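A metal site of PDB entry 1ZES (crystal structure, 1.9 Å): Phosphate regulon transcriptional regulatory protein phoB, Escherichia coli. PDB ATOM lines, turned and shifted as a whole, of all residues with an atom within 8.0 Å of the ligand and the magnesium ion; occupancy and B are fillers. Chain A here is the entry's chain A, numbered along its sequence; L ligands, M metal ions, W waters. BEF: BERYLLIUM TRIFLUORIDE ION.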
ATOM      1  N   VAL A   8      25.921 -23.222   9.155  1.00  0.00           N
ATOM      2  CA  VAL A   8      25.149 -22.890  10.381  1.00  0.00           C
ATOM      3  C   VAL A   8      23.789 -23.516  10.289  1.00  0.00           C
ATOM      4  O   VAL A   8      22.970 -23.118   9.460  1.00  0.00           O
ATOM      5  CB  VAL A   8      25.019 -21.342  10.627  1.00  0.00           C
ATOM      6  CG1 VAL A   8      24.410 -21.052  12.044  1.00  0.00           C
ATOM      7  CG2 VAL A   8      26.398 -20.595  10.418  1.00  0.00           C
ATOM      8  N   GLU A   9      23.548 -24.526  11.118  1.00  0.00           N
ATOM      9  CA  GLU A   9      22.328 -25.329  10.986  1.00  0.00           C
ATOM     10  C   GLU A   9      22.159 -26.114  12.271  1.00  0.00           C
ATOM     11  O   GLU A   9      23.109 -26.781  12.693  1.00  0.00           O
ATOM     12  CB  GLU A   9      22.505 -26.312   9.806  1.00  0.00           C
ATOM     13  CG  GLU A   9      21.515 -27.446   9.761  1.00  0.00           C
ATOM     14  CD  GLU A   9      20.099 -26.969   9.628  1.00  0.00           C
ATOM     15  OE1 GLU A   9      19.800 -26.233   8.654  1.00  0.00           O
ATOM     16  OE2 GLU A   9      19.288 -27.330  10.499  1.00  0.00           O
ATOM     17  N   ASP A  10      20.992 -26.053  12.888  1.00  0.00           N
ATOM     18  CA  ASP A  10      20.821 -26.713  14.198  1.00  0.00           C
ATOM     19  C   ASP A  10      20.356 -28.148  14.177  1.00  0.00           C
ATOM     20  O   ASP A  10      20.438 -28.839  15.184  1.00  0.00           O
ATOM     21  CB  ASP A  10      19.889 -25.902  15.093  1.00  0.00           C
ATOM     22  CG  ASP A  10      18.518 -25.691  14.497  1.00  0.00           C
ATOM     23  OD1 ASP A  10      18.396 -25.361  13.308  1.00  0.00           O
ATOM     24  OD2 ASP A  10      17.534 -25.802  15.259  1.00  0.00           O
ATOM     25  N   GLU A  11      19.827 -28.615  13.039  1.00  0.00           N
ATOM     26  CA  GLU A  11      19.460 -30.022  12.956  1.00  0.00           C
ATOM     27  C   GLU A  11      20.709 -30.776  12.554  1.00  0.00           C
ATOM     28  O   GLU A  11      21.142 -30.701  11.407  1.00  0.00           O
ATOM     29  CB  GLU A  11      18.347 -30.206  11.951  1.00  0.00           C
ATOM     30  CG  GLU A  11      17.055 -29.556  12.426  1.00  0.00           C
ATOM     31  CD  GLU A  11      15.919 -29.715  11.444  1.00  0.00           C
ATOM     32  OE1 GLU A  11      15.680 -30.858  11.009  1.00  0.00           O
ATOM     33  OE2 GLU A  11      15.286 -28.696  11.105  1.00  0.00           O
ATOM     34  N   ILE A  14      20.907 -33.064   9.319  1.00  0.00           N
ATOM     35  CA  ILE A  14      20.911 -32.208   8.126  1.00  0.00           C
ATOM     36  C   ILE A  14      22.254 -31.469   7.962  1.00  0.00           C
ATOM     37  O   ILE A  14      22.805 -31.422   6.883  1.00  0.00           O
ATOM     38  CB  ILE A  14      19.737 -31.211   8.182  1.00  0.00           C
ATOM     39  CG1 ILE A  14      18.400 -32.002   8.302  1.00  0.00           C
ATOM     40  CG2 ILE A  14      19.764 -30.247   6.955  1.00  0.00           C
ATOM     41  CD1 ILE A  14      18.121 -32.932   7.111  1.00  0.00           C
ATOM     42  N   GLU A  33      26.103 -24.909  15.296  1.00  0.00           N
ATOM     43  CA  GLU A  33      24.775 -25.493  15.570  1.00  0.00           C
ATOM     44  C   GLU A  33      23.739 -24.487  16.076  1.00  0.00           C
ATOM     45  O   GLU A  33      22.571 -24.822  16.232  1.00  0.00           O
ATOM     46  CB  GLU A  33      24.888 -26.668  16.557  1.00  0.00           C
ATOM     47  CG  GLU A  33      25.364 -26.268  17.979  1.00  0.00           C
ATOM     48  CD  GLU A  33      25.369 -27.471  18.944  1.00  0.00           C
ATOM     49  OE1 GLU A  33      25.119 -28.621  18.510  1.00  0.00           O
ATOM     50  OE2 GLU A  33      25.632 -27.272  20.142  1.00  0.00           O
ATOM     51  N   LEU A  52      23.723 -20.536   5.751  1.00  0.00           N
ATOM     52  CA  LEU A  52      23.090 -20.118   6.997  1.00  0.00           C
ATOM     53  C   LEU A  52      21.620 -20.505   7.102  1.00  0.00           C
ATOM     54  O   LEU A  52      20.793 -20.066   6.259  1.00  0.00           O
ATOM     55  CB  LEU A  52      23.279 -18.568   7.140  1.00  0.00           C
ATOM     56  CG  LEU A  52      22.475 -17.903   8.258  1.00  0.00           C
ATOM     57  CD1 LEU A  52      23.118 -18.321   9.576  1.00  0.00           C
ATOM     58  CD2 LEU A  52      22.521 -16.388   8.090  1.00  0.00           C
ATOM     59  N   ASP A  53      21.298 -21.321   8.103  1.00  0.00           N
ATOM     60  CA  ASP A  53      19.892 -21.695   8.399  1.00  0.00           C
ATOM     61  C   ASP A  53      19.237 -20.468   9.016  1.00  0.00           C
ATOM     62  O   ASP A  53      19.935 -19.583   9.562  1.00  0.00           O
ATOM     63  CB  ASP A  53      19.874 -22.902   9.345  1.00  0.00           C
ATOM     64  CG  ASP A  53      18.493 -23.397   9.682  1.00  0.00           C
ATOM     65  OD1 ASP A  53      17.532 -23.198   8.922  1.00  0.00           O
ATOM     66  OD2 ASP A  53      18.386 -24.035  10.735  1.00  0.00           O
ATOM     67  N   TRP A  54      17.921 -20.343   8.863  1.00  0.00           N
ATOM     68  CA  TRP A  54      17.213 -19.205   9.468  1.00  0.00           C
ATOM     69  C   TRP A  54      16.864 -19.472  10.948  1.00  0.00           C
ATOM     70  O   TRP A  54      17.344 -18.772  11.861  1.00  0.00           O
ATOM     71  CB  TRP A  54      15.941 -18.907   8.654  1.00  0.00           C
ATOM     72  CG  TRP A  54      15.061 -17.749   9.147  1.00  0.00           C
ATOM     73  CD1 TRP A  54      14.607 -17.528  10.435  1.00  0.00           C
ATOM     74  CD2 TRP A  54      14.484 -16.717   8.340  1.00  0.00           C
ATOM     75  NE1 TRP A  54      13.788 -16.406  10.463  1.00  0.00           N
ATOM     76  CE2 TRP A  54      13.698 -15.889   9.197  1.00  0.00           C
ATOM     77  CE3 TRP A  54      14.558 -16.415   6.966  1.00  0.00           C
ATOM     78  CZ2 TRP A  54      12.998 -14.765   8.729  1.00  0.00           C
ATOM     79  CZ3 TRP A  54      13.873 -15.289   6.511  1.00  0.00           C
ATOM     80  CH2 TRP A  54      13.099 -14.478   7.389  1.00  0.00           C
ATOM     81  N   MET A  55      16.091 -20.516  11.194  1.00  0.00           N
ATOM     82  CA  MET A  55      15.598 -20.824  12.540  1.00  0.00           C
ATOM     83  C   MET A  55      16.639 -21.614  13.320  1.00  0.00           C
ATOM     84  O   MET A  55      16.898 -22.792  13.032  1.00  0.00           O
ATOM     85  CB  MET A  55      14.288 -21.600  12.449  1.00  0.00           C
ATOM     86  CG  MET A  55      13.279 -20.894  11.551  1.00  0.00           C
ATOM     87  SD  MET A  55      11.677 -21.722  11.445  1.00  0.00           S
ATOM     88  CE  MET A  55      12.034 -23.079  10.326  1.00  0.00           C
ATOM     89  N   LEU A  56      17.233 -20.921  14.301  1.00  0.00           N
ATOM     90  CA  LEU A  56      18.351 -21.402  15.116  1.00  0.00           C
ATOM     91  C   LEU A  56      18.117 -21.033  16.568  1.00  0.00           C
ATOM     92  O   LEU A  56      17.537 -19.981  16.827  1.00  0.00           O
ATOM     93  CB  LEU A  56      19.638 -20.704  14.678  1.00  0.00           C
ATOM     94  CG  LEU A  56      20.139 -21.008  13.238  1.00  0.00           C
ATOM     95  CD1 LEU A  56      21.127 -19.965  12.922  1.00  0.00           C
ATOM     96  CD2 LEU A  56      20.807 -22.385  13.159  1.00  0.00           C
ATOM     97  N   PRO A  57      18.574 -21.878  17.514  1.00  0.00           N
ATOM     98  CA  PRO A  57      18.572 -21.495  18.935  1.00  0.00           C
ATOM     99  C   PRO A  57      19.400 -20.251  19.218  1.00  0.00           C
ATOM    100  O   PRO A  57      20.509 -20.091  18.676  1.00  0.00           O
ATOM    101  CB  PRO A  57      19.167 -22.722  19.647  1.00  0.00           C
ATOM    102  CG  PRO A  57      18.917 -23.854  18.699  1.00  0.00           C
ATOM    103  CD  PRO A  57      19.083 -23.256  17.328  1.00  0.00           C
ATOM    104  N   GLY A  61      18.971 -16.532  11.750  1.00  0.00           N
ATOM    105  CA  GLY A  61      19.973 -16.200  10.764  1.00  0.00           C
ATOM    106  C   GLY A  61      19.843 -14.763  10.254  1.00  0.00           C
ATOM    107  O   GLY A  61      20.846 -14.182   9.836  1.00  0.00           O
ATOM    108  N   MET A  81      21.542 -18.158   2.437  1.00  0.00           N
ATOM    109  CA  MET A  81      20.647 -18.813   3.405  1.00  0.00           C
ATOM    110  C   MET A  81      20.133 -20.148   2.851  1.00  0.00           C
ATOM    111  O   MET A  81      19.984 -20.302   1.649  1.00  0.00           O
ATOM    112  CB  MET A  81      19.515 -17.885   3.805  1.00  0.00           C
ATOM    113  CG  MET A  81      20.009 -16.620   4.539  1.00  0.00           C
ATOM    114  SD  MET A  81      18.663 -15.680   5.278  1.00  0.00           S
ATOM    115  CE  MET A  81      18.357 -16.668   6.739  1.00  0.00           C
ATOM    116  N   LEU A  82      19.919 -21.119   3.735  1.00  0.00           N
ATOM    117  CA  LEU A  82      19.392 -22.427   3.335  1.00  0.00           C
ATOM    118  C   LEU A  82      18.436 -22.827   4.454  1.00  0.00           C
ATOM    119  O   LEU A  82      18.857 -23.105   5.571  1.00  0.00           O
ATOM    120  CB  LEU A  82      20.559 -23.415   3.207  1.00  0.00           C
ATOM    121  CG  LEU A  82      20.211 -24.887   2.955  1.00  0.00           C
ATOM    122  CD1 LEU A  82      19.412 -25.027   1.668  1.00  0.00           C
ATOM    123  CD2 LEU A  82      21.463 -25.754   2.936  1.00  0.00           C
ATOM    124  N   THR A  83      17.147 -22.819   4.165  1.00  0.00           N
ATOM    125  CA  THR A  83      16.154 -22.755   5.236  1.00  0.00           C
ATOM    126  C   THR A  83      14.834 -23.312   4.795  1.00  0.00           C
ATOM    127  O   THR A  83      14.454 -23.236   3.622  1.00  0.00           O
ATOM    128  CB  THR A  83      15.857 -21.278   5.716  1.00  0.00           C
ATOM    129  OG1 THR A  83      14.669 -21.298   6.533  1.00  0.00           O
ATOM    130  CG2 THR A  83      15.568 -20.351   4.516  1.00  0.00           C
ATOM    131  N   ALA A  84      14.077 -23.812   5.771  1.00  0.00           N
ATOM    132  CA  ALA A  84      12.733 -24.296   5.503  1.00  0.00           C
ATOM    133  C   ALA A  84      11.686 -23.175   5.348  1.00  0.00           C
ATOM    134  O   ALA A  84      10.532 -23.432   4.962  1.00  0.00           O
ATOM    135  CB  ALA A  84      12.322 -25.247   6.608  1.00  0.00           C
ATOM    136  N   ARG A  85      12.079 -21.936   5.655  1.00  0.00           N
ATOM    137  CA  ARG A  85      11.200 -20.766   5.476  1.00  0.00           C
ATOM    138  C   ARG A  85      11.152 -20.378   3.995  1.00  0.00           C
ATOM    139  O   ARG A  85      12.032 -19.640   3.505  1.00  0.00           O
ATOM    140  CB  ARG A  85      11.665 -19.585   6.310  1.00  0.00           C
ATOM    141  CG  ARG A  85      11.567 -19.882   7.793  1.00  0.00           C
ATOM    142  CD  ARG A  85      11.662 -18.637   8.668  1.00  0.00           C
ATOM    143  NE  ARG A  85      10.391 -17.926   8.742  1.00  0.00           N
ATOM    144  CZ  ARG A  85       9.476 -18.088   9.700  1.00  0.00           C
ATOM    145  NH1 ARG A  85       9.656 -18.954  10.686  1.00  0.00           N
ATOM    146  NH2 ARG A  85       8.361 -17.368   9.643  1.00  0.00           N
ATOM    147  N   GLY A  86      10.117 -20.866   3.336  1.00  0.00           N
ATOM    148  CA  GLY A  86       9.958 -20.715   1.910  1.00  0.00           C
ATOM    149  C   GLY A  86       8.998 -19.670   1.393  1.00  0.00           C
ATOM    150  O   GLY A  86       8.941 -19.461   0.165  1.00  0.00           O
ATOM    151  N   TYR A 102      19.412 -17.222  -1.337  1.00  0.00           N
ATOM    152  CA  TYR A 102      18.452 -17.744  -0.379  1.00  0.00           C
ATOM    153  C   TYR A 102      17.870 -18.997  -0.993  1.00  0.00           C
ATOM    154  O   TYR A 102      17.177 -18.935  -2.037  1.00  0.00           O
ATOM    155  CB  TYR A 102      17.373 -16.665  -0.154  1.00  0.00           C
ATOM    156  CG  TYR A 102      16.384 -16.944   0.965  1.00  0.00           C
ATOM    157  CD1 TYR A 102      15.441 -17.956   0.838  1.00  0.00           C
ATOM    158  CD2 TYR A 102      16.404 -16.187   2.141  1.00  0.00           C
ATOM    159  CE1 TYR A 102      14.516 -18.208   1.858  1.00  0.00           C
ATOM    160  CE2 TYR A 102      15.461 -16.450   3.185  1.00  0.00           C
ATOM    161  CZ  TYR A 102      14.542 -17.475   3.015  1.00  0.00           C
ATOM    162  OH  TYR A 102      13.593 -17.743   3.989  1.00  0.00           O
ATOM    163  N   ILE A 103      18.167 -20.150  -0.395  1.00  0.00           N
ATOM    164  CA  ILE A 103      17.712 -21.445  -0.932  1.00  0.00           C
ATOM    165  C   ILE A 103      16.788 -22.132   0.062  1.00  0.00           C
ATOM    166  O   ILE A 103      17.039 -22.102   1.276  1.00  0.00           O
ATOM    167  CB  ILE A 103      18.915 -22.392  -1.241  1.00  0.00           C
ATOM    168  CG1 ILE A 103      19.889 -21.688  -2.187  1.00  0.00           C
ATOM    169  CG2 ILE A 103      18.429 -23.707  -1.895  1.00  0.00           C
ATOM    170  CD1 ILE A 103      21.298 -22.392  -2.239  1.00  0.00           C
ATOM    171  N   THR A 104      15.700 -22.732  -0.447  1.00  0.00           N
ATOM    172  CA  THR A 104      14.685 -23.302   0.443  1.00  0.00           C
ATOM    173  C   THR A 104      14.884 -24.813   0.567  1.00  0.00           C
ATOM    174  O   THR A 104      15.311 -25.452  -0.399  1.00  0.00           O
ATOM    175  CB  THR A 104      13.274 -23.079  -0.122  1.00  0.00           C
ATOM    176  OG1 THR A 104      13.267 -23.566  -1.479  1.00  0.00           O
ATOM    177  CG2 THR A 104      12.924 -21.628  -0.159  1.00  0.00           C
ATOM    178  N   LYS A 105      14.597 -25.368   1.743  1.00  0.00           N
ATOM    179  CA  LYS A 105      14.569 -26.818   1.955  1.00  0.00           C
ATOM    180  C   LYS A 105      13.187 -27.354   1.522  1.00  0.00           C
ATOM    181  O   LYS A 105      12.179 -26.702   1.763  1.00  0.00           O
ATOM    182  CB  LYS A 105      14.729 -27.144   3.447  1.00  0.00           C
ATOM    183  CG  LYS A 105      16.122 -26.957   4.063  1.00  0.00           C
ATOM    184  CD  LYS A 105      16.035 -27.095   5.596  1.00  0.00           C
ATOM    185  CE  LYS A 105      17.324 -26.685   6.231  1.00  0.00           C
ATOM    186  NZ  LYS A 105      17.241 -26.492   7.725  1.00  0.00           N
HETATM  187 BE   BEF L   1      15.865 -23.488   9.153  1.00  0.00          BE
HETATM  188  F1  BEF L   1      15.533 -23.866  10.572  1.00  0.00           F
HETATM  189  F2  BEF L   1      15.248 -22.156   8.797  1.00  0.00           F
HETATM  190  F3  BEF L   1      15.337 -24.543   8.227  1.00  0.00           F
HETATM  191 MG    MG M   1      16.983 -24.566  12.027  1.00  0.00          MG
HETATM  192  O   HOH W   1      16.991 -26.499  11.020  1.00  0.00           O
HETATM  193  O   HOH W   2      13.660 -26.214   9.764  1.00  0.00           O
HETATM  194  O   HOH W   3      15.371 -25.328  13.255  1.00  0.00           O
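OD1 of Asp 53 is bound to BE of the ligand, 1.7 Å away. The backbone NH (N) of Met 55 lies within hydrogen-bond range of a fluorine (F2) of the ligand (3.0 Å). A fluorine (F2) of the ligand sits at hydrogen-bond distance from the side-chain hydroxyl (OG1) of Thr 83, 2.5 Å away. The side-chain amino group of Lys 105 lies within hydrogen-bond range of a fluorine (F3) of the ligand (2.8 Å). The backbone NH (N) of Ala 84 lies within hydrogen-bond range of a fluorine (F3) of the ligand. The backbone NH (N) of Trp 54 is in hydrogen-bond range of a fluorine (F2) of the ligand (3.2 Å).
O of Val 8 sits at hydrogen-bond distance from N of Asp 53. The guanidinium group of Arg 85 is in hydrogen-bond range of the side-chain sulfur of Met 55 (3.5 Å). The backbone NH (N) of Lys 105 sits at hydrogen-bond distance from the backbone carbonyl oxygen (O) of Thr 83. OG1 of Thr 83 sits at hydrogen-bond distance from N of Arg 85 (2.8 Å). The backbone NH (N) of Thr 83 lies within hydrogen-bond range of the backbone carbonyl oxygen (O) of Ile 103. The side-chain carboxylate (OE1) of Glu 9 lies within salt-bridge range of the side-chain amino group (NZ) of Lys 105. The backbone NH (N) of Gly 61 is in hydrogen-bond range of the backbone carbonyl oxygen (O) of Trp 54 (2.8 Å). The side-chain carboxylate (OE2) of Glu 9 sits at hydrogen-bond distance from the backbone NH (N) of Glu 11.
Hydrophobic or aromatic side chains within 4 Å of the ligand: Trp 54, Met 55 and Ala 84. Within 4 Å of the ligand: Asp 53, Trp 54, Met 55, Thr 83, Ala 84 and Lys 105.
Glu 9 touches the magnesium ion (OE2 to MG, 3.9 Å). Of the 23 residues printed, 4 come within 4 Å of the magnesium ion. The nearest printed residue that does not touch the magnesium ion is Leu 56 (4.3 Å).
The magnesium ion is bound by OD2 of Asp 53, O of Met 55, OD1 of Asp 10, water W3, F1 of the ligand and water W1. The magnesium ion has six donor atoms within binding distance.
Water W1 lies within hydrogen-bond range of OE2 of Glu 9 (2.5 Å), OE2 of Glu 11 (2.8 Å) and NZ of Lys 105 (3.3 Å). Water W2 lies within hydrogen-bond range of a fluorine (F3) of the ligand (2.8 Å) and the side-chain carboxylate (OE2) of Glu 11 (3.3 Å).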
